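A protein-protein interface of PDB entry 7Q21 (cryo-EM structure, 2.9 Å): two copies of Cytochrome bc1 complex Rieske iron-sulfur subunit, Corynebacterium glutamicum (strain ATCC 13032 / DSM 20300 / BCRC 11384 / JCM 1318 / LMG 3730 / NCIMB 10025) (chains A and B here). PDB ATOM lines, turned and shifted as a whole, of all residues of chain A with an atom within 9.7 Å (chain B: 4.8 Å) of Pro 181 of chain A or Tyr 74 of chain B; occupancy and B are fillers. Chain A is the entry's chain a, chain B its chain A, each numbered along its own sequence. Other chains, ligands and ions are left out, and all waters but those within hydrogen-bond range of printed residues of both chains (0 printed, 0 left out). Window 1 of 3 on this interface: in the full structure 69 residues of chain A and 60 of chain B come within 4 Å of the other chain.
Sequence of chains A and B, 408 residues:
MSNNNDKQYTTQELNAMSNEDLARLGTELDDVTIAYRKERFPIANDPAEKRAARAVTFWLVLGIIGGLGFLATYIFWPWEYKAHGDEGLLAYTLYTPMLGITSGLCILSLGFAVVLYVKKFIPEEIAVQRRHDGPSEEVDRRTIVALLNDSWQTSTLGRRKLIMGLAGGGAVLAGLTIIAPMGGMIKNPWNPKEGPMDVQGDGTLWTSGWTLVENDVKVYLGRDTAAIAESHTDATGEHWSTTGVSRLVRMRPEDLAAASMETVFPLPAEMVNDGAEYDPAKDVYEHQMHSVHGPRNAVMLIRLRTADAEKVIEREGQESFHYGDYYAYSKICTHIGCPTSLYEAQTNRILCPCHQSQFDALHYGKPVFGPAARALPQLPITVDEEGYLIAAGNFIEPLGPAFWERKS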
ATOM      1  N   LEU A 173     -20.816 -25.387 -13.566  1.00  0.00           N
ATOM      2  CA  LEU A 173     -21.932 -24.475 -13.372  1.00  0.00           C
ATOM      3  C   LEU A 173     -22.338 -24.415 -11.902  1.00  0.00           C
ATOM      4  O   LEU A 173     -22.644 -23.332 -11.406  1.00  0.00           O
ATOM      5  CB  LEU A 173     -23.105 -24.867 -14.274  1.00  0.00           C
ATOM      6  CG  LEU A 173     -23.009 -24.368 -15.714  1.00  0.00           C
ATOM      7  CD1 LEU A 173     -24.225 -24.802 -16.514  1.00  0.00           C
ATOM      8  CD2 LEU A 173     -22.855 -22.855 -15.754  1.00  0.00           C
ATOM      9  N   ALA A 174     -22.307 -25.572 -11.219  1.00  0.00           N
ATOM     10  CA  ALA A 174     -22.602 -25.633  -9.794  1.00  0.00           C
ATOM     11  C   ALA A 174     -21.580 -24.810  -9.018  1.00  0.00           C
ATOM     12  O   ALA A 174     -21.967 -23.911  -8.273  1.00  0.00           O
ATOM     13  CB  ALA A 174     -22.649 -27.059  -9.311  1.00  0.00           C
ATOM     14  N   GLY A 175     -20.294 -25.042  -9.304  1.00  0.00           N
ATOM     15  CA  GLY A 175     -19.203 -24.353  -8.638  1.00  0.00           C
ATOM     16  C   GLY A 175     -19.311 -22.841  -8.786  1.00  0.00           C
ATOM     17  O   GLY A 175     -19.110 -22.123  -7.811  1.00  0.00           O
ATOM     18  N   LEU A 176     -19.657 -22.380  -9.999  1.00  0.00           N
ATOM     19  CA  LEU A 176     -19.779 -20.947 -10.209  1.00  0.00           C
ATOM     20  C   LEU A 176     -21.150 -20.399  -9.798  1.00  0.00           C
ATOM     21  O   LEU A 176     -21.378 -19.202  -9.947  1.00  0.00           O
ATOM     22  CB  LEU A 176     -19.258 -20.500 -11.587  1.00  0.00           C
ATOM     23  CG  LEU A 176     -20.045 -20.926 -12.822  1.00  0.00           C
ATOM     24  CD1 LEU A 176     -21.062 -19.863 -13.176  1.00  0.00           C
ATOM     25  CD2 LEU A 176     -19.101 -21.135 -13.997  1.00  0.00           C
ATOM     26  N   THR A 177     -22.079 -21.295  -9.419  1.00  0.00           N
ATOM     27  CA  THR A 177     -23.345 -20.913  -8.804  1.00  0.00           C
ATOM     28  C   THR A 177     -23.119 -20.538  -7.339  1.00  0.00           C
ATOM     29  O   THR A 177     -23.759 -19.609  -6.840  1.00  0.00           O
ATOM     30  CB  THR A 177     -24.399 -22.022  -8.959  1.00  0.00           C
ATOM     31  OG1 THR A 177     -24.716 -22.159 -10.341  1.00  0.00           O
ATOM     32  CG2 THR A 177     -25.659 -21.806  -8.152  1.00  0.00           C
ATOM     33  N   ILE A 178     -22.225 -21.268  -6.653  1.00  0.00           N
ATOM     34  CA  ILE A 178     -21.868 -20.970  -5.271  1.00  0.00           C
ATOM     35  C   ILE A 178     -21.222 -19.586  -5.182  1.00  0.00           C
ATOM     36  O   ILE A 178     -21.583 -18.795  -4.320  1.00  0.00           O
ATOM     37  CB  ILE A 178     -20.979 -22.079  -4.659  1.00  0.00           C
ATOM     38  CG1 ILE A 178     -21.769 -23.356  -4.370  1.00  0.00           C
ATOM     39  CG2 ILE A 178     -20.247 -21.598  -3.415  1.00  0.00           C
ATOM     40  CD1 ILE A 178     -21.571 -24.436  -5.406  1.00  0.00           C
ATOM     41  N   ILE A 179     -20.293 -19.285  -6.091  1.00  0.00           N
ATOM     42  CA  ILE A 179     -19.482 -18.080  -5.993  1.00  0.00           C
ATOM     43  C   ILE A 179     -20.145 -16.897  -6.700  1.00  0.00           C
ATOM     44  O   ILE A 179     -19.583 -15.807  -6.689  1.00  0.00           O
ATOM     45  CB  ILE A 179     -18.051 -18.323  -6.517  1.00  0.00           C
ATOM     46  CG1 ILE A 179     -18.065 -18.605  -8.025  1.00  0.00           C
ATOM     47  CG2 ILE A 179     -17.359 -19.411  -5.701  1.00  0.00           C
ATOM     48  CD1 ILE A 179     -16.719 -18.533  -8.706  1.00  0.00           C
ATOM     49  N   ALA A 180     -21.310 -17.099  -7.331  1.00  0.00           N
ATOM     50  CA  ALA A 180     -21.965 -16.024  -8.068  1.00  0.00           C
ATOM     51  C   ALA A 180     -22.381 -14.864  -7.153  1.00  0.00           C
ATOM     52  O   ALA A 180     -22.121 -13.711  -7.493  1.00  0.00           O
ATOM     53  CB  ALA A 180     -23.101 -16.540  -8.918  1.00  0.00           C
ATOM     54  N   PRO A 181     -23.014 -15.089  -5.972  1.00  0.00           N
ATOM     55  CA  PRO A 181     -23.368 -13.985  -5.075  1.00  0.00           C
ATOM     56  C   PRO A 181     -22.204 -13.128  -4.578  1.00  0.00           C
ATOM     57  O   PRO A 181     -22.420 -12.163  -3.857  1.00  0.00           O
ATOM     58  CB  PRO A 181     -24.106 -14.644  -3.906  1.00  0.00           C
ATOM     59  CG  PRO A 181     -23.673 -16.076  -3.967  1.00  0.00           C
ATOM     60  CD  PRO A 181     -23.491 -16.377  -5.440  1.00  0.00           C
ATOM     61  N   MET A 182     -20.975 -13.464  -4.990  1.00  0.00           N
ATOM     62  CA  MET A 182     -19.818 -12.605  -4.784  1.00  0.00           C
ATOM     63  C   MET A 182     -19.886 -11.371  -5.690  1.00  0.00           C
ATOM     64  O   MET A 182     -19.067 -10.469  -5.548  1.00  0.00           O
ATOM     65  CB  MET A 182     -18.517 -13.373  -5.018  1.00  0.00           C
ATOM     66  CG  MET A 182     -18.043 -14.087  -3.772  1.00  0.00           C
ATOM     67  SD  MET A 182     -17.362 -12.841  -2.650  1.00  0.00           S
ATOM     68  CE  MET A 182     -17.396 -13.719  -1.091  1.00  0.00           C
ATOM     69  N   GLY A 183     -20.862 -11.339  -6.608  1.00  0.00           N
ATOM     70  CA  GLY A 183     -21.151 -10.179  -7.436  1.00  0.00           C
ATOM     71  C   GLY A 183     -21.847  -9.051  -6.673  1.00  0.00           C
ATOM     72  O   GLY A 183     -22.051  -7.963  -7.209  1.00  0.00           O
ATOM     73  N   GLY A 184     -22.249  -9.336  -5.430  1.00  0.00           N
ATOM     74  CA  GLY A 184     -22.796  -8.344  -4.518  1.00  0.00           C
ATOM     75  C   GLY A 184     -21.725  -7.359  -4.061  1.00  0.00           C
ATOM     76  O   GLY A 184     -22.037  -6.251  -3.621  1.00  0.00           O
ATOM     77  N   MET A 185     -20.461  -7.789  -4.169  1.00  0.00           N
ATOM     78  CA  MET A 185     -19.334  -6.936  -3.832  1.00  0.00           C
ATOM     79  C   MET A 185     -19.009  -5.997  -4.991  1.00  0.00           C
ATOM     80  O   MET A 185     -18.492  -4.908  -4.750  1.00  0.00           O
ATOM     81  CB  MET A 185     -18.097  -7.749  -3.452  1.00  0.00           C
ATOM     82  CG  MET A 185     -18.203  -8.355  -2.072  1.00  0.00           C
ATOM     83  SD  MET A 185     -16.735  -9.328  -1.686  1.00  0.00           S
ATOM     84  CE  MET A 185     -15.648  -8.059  -1.039  1.00  0.00           C
ATOM     85  N   ILE A 186     -19.319  -6.421  -6.227  1.00  0.00           N
ATOM     86  CA  ILE A 186     -19.069  -5.623  -7.419  1.00  0.00           C
ATOM     87  C   ILE A 186     -19.853  -4.316  -7.325  1.00  0.00           C
ATOM     88  O   ILE A 186     -21.052  -4.312  -7.053  1.00  0.00           O
ATOM     89  CB  ILE A 186     -19.404  -6.391  -8.719  1.00  0.00           C
ATOM     90  CG1 ILE A 186     -18.648  -7.717  -8.846  1.00  0.00           C
ATOM     91  CG2 ILE A 186     -19.235  -5.506  -9.949  1.00  0.00           C
ATOM     92  CD1 ILE A 186     -17.184  -7.581  -9.174  1.00  0.00           C
ATOM     93  N   GLY B  69     -29.876 -20.745 -15.722  1.00  0.00           N
ATOM     94  CA  GLY B  69     -31.005 -19.986 -15.206  1.00  0.00           C
ATOM     95  C   GLY B  69     -30.612 -19.113 -14.015  1.00  0.00           C
ATOM     96  O   GLY B  69     -30.969 -17.941 -13.954  1.00  0.00           O
ATOM     97  N   PHE B  70     -29.854 -19.703 -13.081  1.00  0.00           N
ATOM     98  CA  PHE B  70     -29.404 -18.986 -11.900  1.00  0.00           C
ATOM     99  C   PHE B  70     -28.511 -17.818 -12.297  1.00  0.00           C
ATOM    100  O   PHE B  70     -28.646 -16.739 -11.731  1.00  0.00           O
ATOM    101  CB  PHE B  70     -28.700 -19.901 -10.894  1.00  0.00           C
ATOM    102  CG  PHE B  70     -28.183 -19.177  -9.676  1.00  0.00           C
ATOM    103  CD1 PHE B  70     -28.999 -18.975  -8.570  1.00  0.00           C
ATOM    104  CD2 PHE B  70     -26.891 -18.671  -9.643  1.00  0.00           C
ATOM    105  CE1 PHE B  70     -28.532 -18.296  -7.452  1.00  0.00           C
ATOM    106  CE2 PHE B  70     -26.424 -17.992  -8.527  1.00  0.00           C
ATOM    107  CZ  PHE B  70     -27.242 -17.809  -7.431  1.00  0.00           C
ATOM    108  N   LEU B  71     -27.595 -18.050 -13.246  1.00  0.00           N
ATOM    109  CA  LEU B  71     -26.699 -16.993 -13.685  1.00  0.00           C
ATOM    110  C   LEU B  71     -27.491 -15.878 -14.361  1.00  0.00           C
ATOM    111  O   LEU B  71     -27.250 -14.708 -14.076  1.00  0.00           O
ATOM    112  CB  LEU B  71     -25.626 -17.562 -14.617  1.00  0.00           C
ATOM    113  CG  LEU B  71     -24.509 -18.363 -13.955  1.00  0.00           C
ATOM    114  CD1 LEU B  71     -23.485 -18.774 -15.004  1.00  0.00           C
ATOM    115  CD2 LEU B  71     -23.852 -17.563 -12.837  1.00  0.00           C
ATOM    116  N   ALA B  72     -28.454 -16.258 -15.213  1.00  0.00           N
ATOM    117  CA  ALA B  72     -29.236 -15.299 -15.977  1.00  0.00           C
ATOM    118  C   ALA B  72     -30.141 -14.485 -15.056  1.00  0.00           C
ATOM    119  O   ALA B  72     -30.275 -13.277 -15.248  1.00  0.00           O
ATOM    120  CB  ALA B  72     -30.019 -15.988 -17.068  1.00  0.00           C
ATOM    121  N   THR B  73     -30.730 -15.134 -14.044  1.00  0.00           N
ATOM    122  CA  THR B  73     -31.634 -14.437 -13.141  1.00  0.00           C
ATOM    123  C   THR B  73     -30.843 -13.531 -12.200  1.00  0.00           C
ATOM    124  O   THR B  73     -31.275 -12.410 -11.935  1.00  0.00           O
ATOM    125  CB  THR B  73     -32.554 -15.383 -12.356  1.00  0.00           C
ATOM    126  OG1 THR B  73     -31.740 -16.212 -11.526  1.00  0.00           O
ATOM    127  CG2 THR B  73     -33.493 -16.206 -13.214  1.00  0.00           C
ATOM    128  N   TYR B  74     -29.675 -14.007 -11.744  1.00  0.00           N
ATOM    129  CA  TYR B  74     -28.856 -13.247 -10.812  1.00  0.00           C
ATOM    130  C   TYR B  74     -28.410 -11.935 -11.460  1.00  0.00           C
ATOM    131  O   TYR B  74     -28.418 -10.894 -10.813  1.00  0.00           O
ATOM    132  CB  TYR B  74     -27.681 -14.084 -10.283  1.00  0.00           C
ATOM    133  CG  TYR B  74     -26.825 -13.382  -9.257  1.00  0.00           C
ATOM    134  CD1 TYR B  74     -25.668 -12.712  -9.629  1.00  0.00           C
ATOM    135  CD2 TYR B  74     -27.195 -13.345  -7.916  1.00  0.00           C
ATOM    136  CE1 TYR B  74     -24.901 -12.022  -8.703  1.00  0.00           C
ATOM    137  CE2 TYR B  74     -26.445 -12.650  -6.979  1.00  0.00           C
ATOM    138  CZ  TYR B  74     -25.289 -11.995  -7.374  1.00  0.00           C
ATOM    139  OH  TYR B  74     -24.525 -11.321  -6.466  1.00  0.00           O
ATOM    140  N   ILE B  75     -28.048 -11.997 -12.753  1.00  0.00           N
ATOM    141  CA  ILE B  75     -27.538 -10.839 -13.465  1.00  0.00           C
ATOM    142  C   ILE B  75     -28.690  -9.926 -13.889  1.00  0.00           C
ATOM    143  O   ILE B  75     -28.693  -8.756 -13.518  1.00  0.00           O
ATOM    144  CB  ILE B  75     -26.624 -11.253 -14.640  1.00  0.00           C
ATOM    145  CG1 ILE B  75     -25.504 -12.187 -14.167  1.00  0.00           C
ATOM    146  CG2 ILE B  75     -26.041 -10.031 -15.339  1.00  0.00           C
ATOM    147  CD1 ILE B  75     -24.723 -12.864 -15.276  1.00  0.00           C
ATOM    148  N   PHE B  76     -29.655 -10.457 -14.650  1.00  0.00           N
ATOM    149  CA  PHE B  76     -30.583  -9.623 -15.397  1.00  0.00           C
ATOM    150  C   PHE B  76     -31.929  -9.351 -14.723  1.00  0.00           C
ATOM    151  O   PHE B  76     -32.597  -8.402 -15.135  1.00  0.00           O
ATOM    152  CB  PHE B  76     -30.767 -10.165 -16.813  1.00  0.00           C
ATOM    153  CG  PHE B  76     -29.485 -10.383 -17.573  1.00  0.00           C
ATOM    154  CD1 PHE B  76     -28.807  -9.314 -18.145  1.00  0.00           C
ATOM    155  CD2 PHE B  76     -28.964 -11.660 -17.737  1.00  0.00           C
ATOM    156  CE1 PHE B  76     -27.626  -9.512 -18.847  1.00  0.00           C
ATOM    157  CE2 PHE B  76     -27.783 -11.859 -18.442  1.00  0.00           C
ATOM    158  CZ  PHE B  76     -27.115 -10.785 -18.991  1.00  0.00           C
ATOM    159  N   TYR B  95     -37.456 -12.106  -6.968  1.00  0.00           N
ATOM    160  CA  TYR B  95     -36.032 -12.223  -7.246  1.00  0.00           C
ATOM    161  C   TYR B  95     -35.401 -13.330  -6.412  1.00  0.00           C
ATOM    162  O   TYR B  95     -34.790 -14.246  -6.956  1.00  0.00           O
ATOM    163  CB  TYR B  95     -35.310 -10.886  -7.069  1.00  0.00           C
ATOM    164  CG  TYR B  95     -33.848 -10.932  -7.435  1.00  0.00           C
ATOM    165  CD1 TYR B  95     -33.463 -10.948  -8.767  1.00  0.00           C
ATOM    166  CD2 TYR B  95     -32.850 -10.961  -6.468  1.00  0.00           C
ATOM    167  CE1 TYR B  95     -32.132 -10.973  -9.136  1.00  0.00           C
ATOM    168  CE2 TYR B  95     -31.509 -11.003  -6.822  1.00  0.00           C
ATOM    169  CZ  TYR B  95     -31.151 -11.015  -8.161  1.00  0.00           C
ATOM    170  OH  TYR B  95     -29.842 -11.042  -8.542  1.00  0.00           O
ATOM    171  N   LEU B  99     -33.967 -17.073  -7.467  1.00  0.00           N
ATOM    172  CA  LEU B  99     -32.614 -17.499  -7.135  1.00  0.00           C
ATOM    173  C   LEU B  99     -32.662 -18.870  -6.466  1.00  0.00           C
ATOM    174  O   LEU B  99     -31.892 -19.753  -6.826  1.00  0.00           O
ATOM    175  CB  LEU B  99     -31.938 -16.485  -6.207  1.00  0.00           C
ATOM    176  CG  LEU B  99     -31.384 -15.200  -6.831  1.00  0.00           C
ATOM    177  CD1 LEU B  99     -30.368 -14.577  -5.886  1.00  0.00           C
ATOM    178  CD2 LEU B  99     -30.739 -15.427  -8.199  1.00  0.00           C
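OG1 of Thr 73 of chain B lies within hydrogen-bond range of O of Phe 70 of chain B, 3.1 Å away.
The backbone carbonyl oxygen (O) of Tyr 74 of chain B is in hydrogen-bond range of the side-chain hydroxyl (OH) of Tyr 95 of chain B (2.7 Å).
The backbone carbonyl oxygen of Leu 173 of chain A lies within hydrogen-bond range of the side-chain hydroxyl of Thr 177 of chain A, 2.6 Å away.
No position is printed for both chains.
Of the 7 pairs that touch across the chains among the printed residues, none has its exchanged pair printed and touching as well.
OH of Tyr 74 of chain B sits close to O of Pro 181 of chain A.
The side-chain hydroxyl of Tyr 74 of chain B sits at hydrogen-bond distance from the backbone NH of Gly 184 of chain A, at 3.2 Å.
Among the printed residues, pairs that only touch across the chains: Leu 176 of chain A with Leu 71 of chain B (3.2 Å), Ala 180 of chain A with Tyr 74 of chain B (3.5 Å), Gly 183 of chain A with Tyr 74 of chain B (3.5 Å), Thr 177 of chain A with Phe 70 of chain B (3.5 Å) and Ala 180 of chain A with Phe 70 of chain B (3.6 Å).
Hydrophobic or aromatic side chains of chain B within 4 Å of the printed part of chain A: Phe 70, Leu 71 and Tyr 74.
Among the printed residues, no Asp or Glu carboxylate lies within 4 Å of a Lys or Arg side-chain nitrogen of the other chain.
Ala 174 of chain A touches none of the printed residues of chain B.
Of the printed residues of chain B, Ala 180 of chain A touches Phe 70 (3.6 Å) and Tyr 74 (3.5 Å).
Of the printed residues of chain A, Phe 70 of chain B touches Thr 177 and Ala 180.
No residue of chain A comes within 4 Å of Thr 73 of chain B.
Ile 75 of chain B touches none of the printed residues of chain A.
Phe 76 of chain B touches none of the printed residues of chain A.
The nearest residue of chain B that does not touch Pro 181 of chain A is Phe 70 of chain B (4.5 Å).
The nearest printed residue of chain A that does not touch Phe 70 of chain B is Pro 181 of chain A (4.5 Å).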
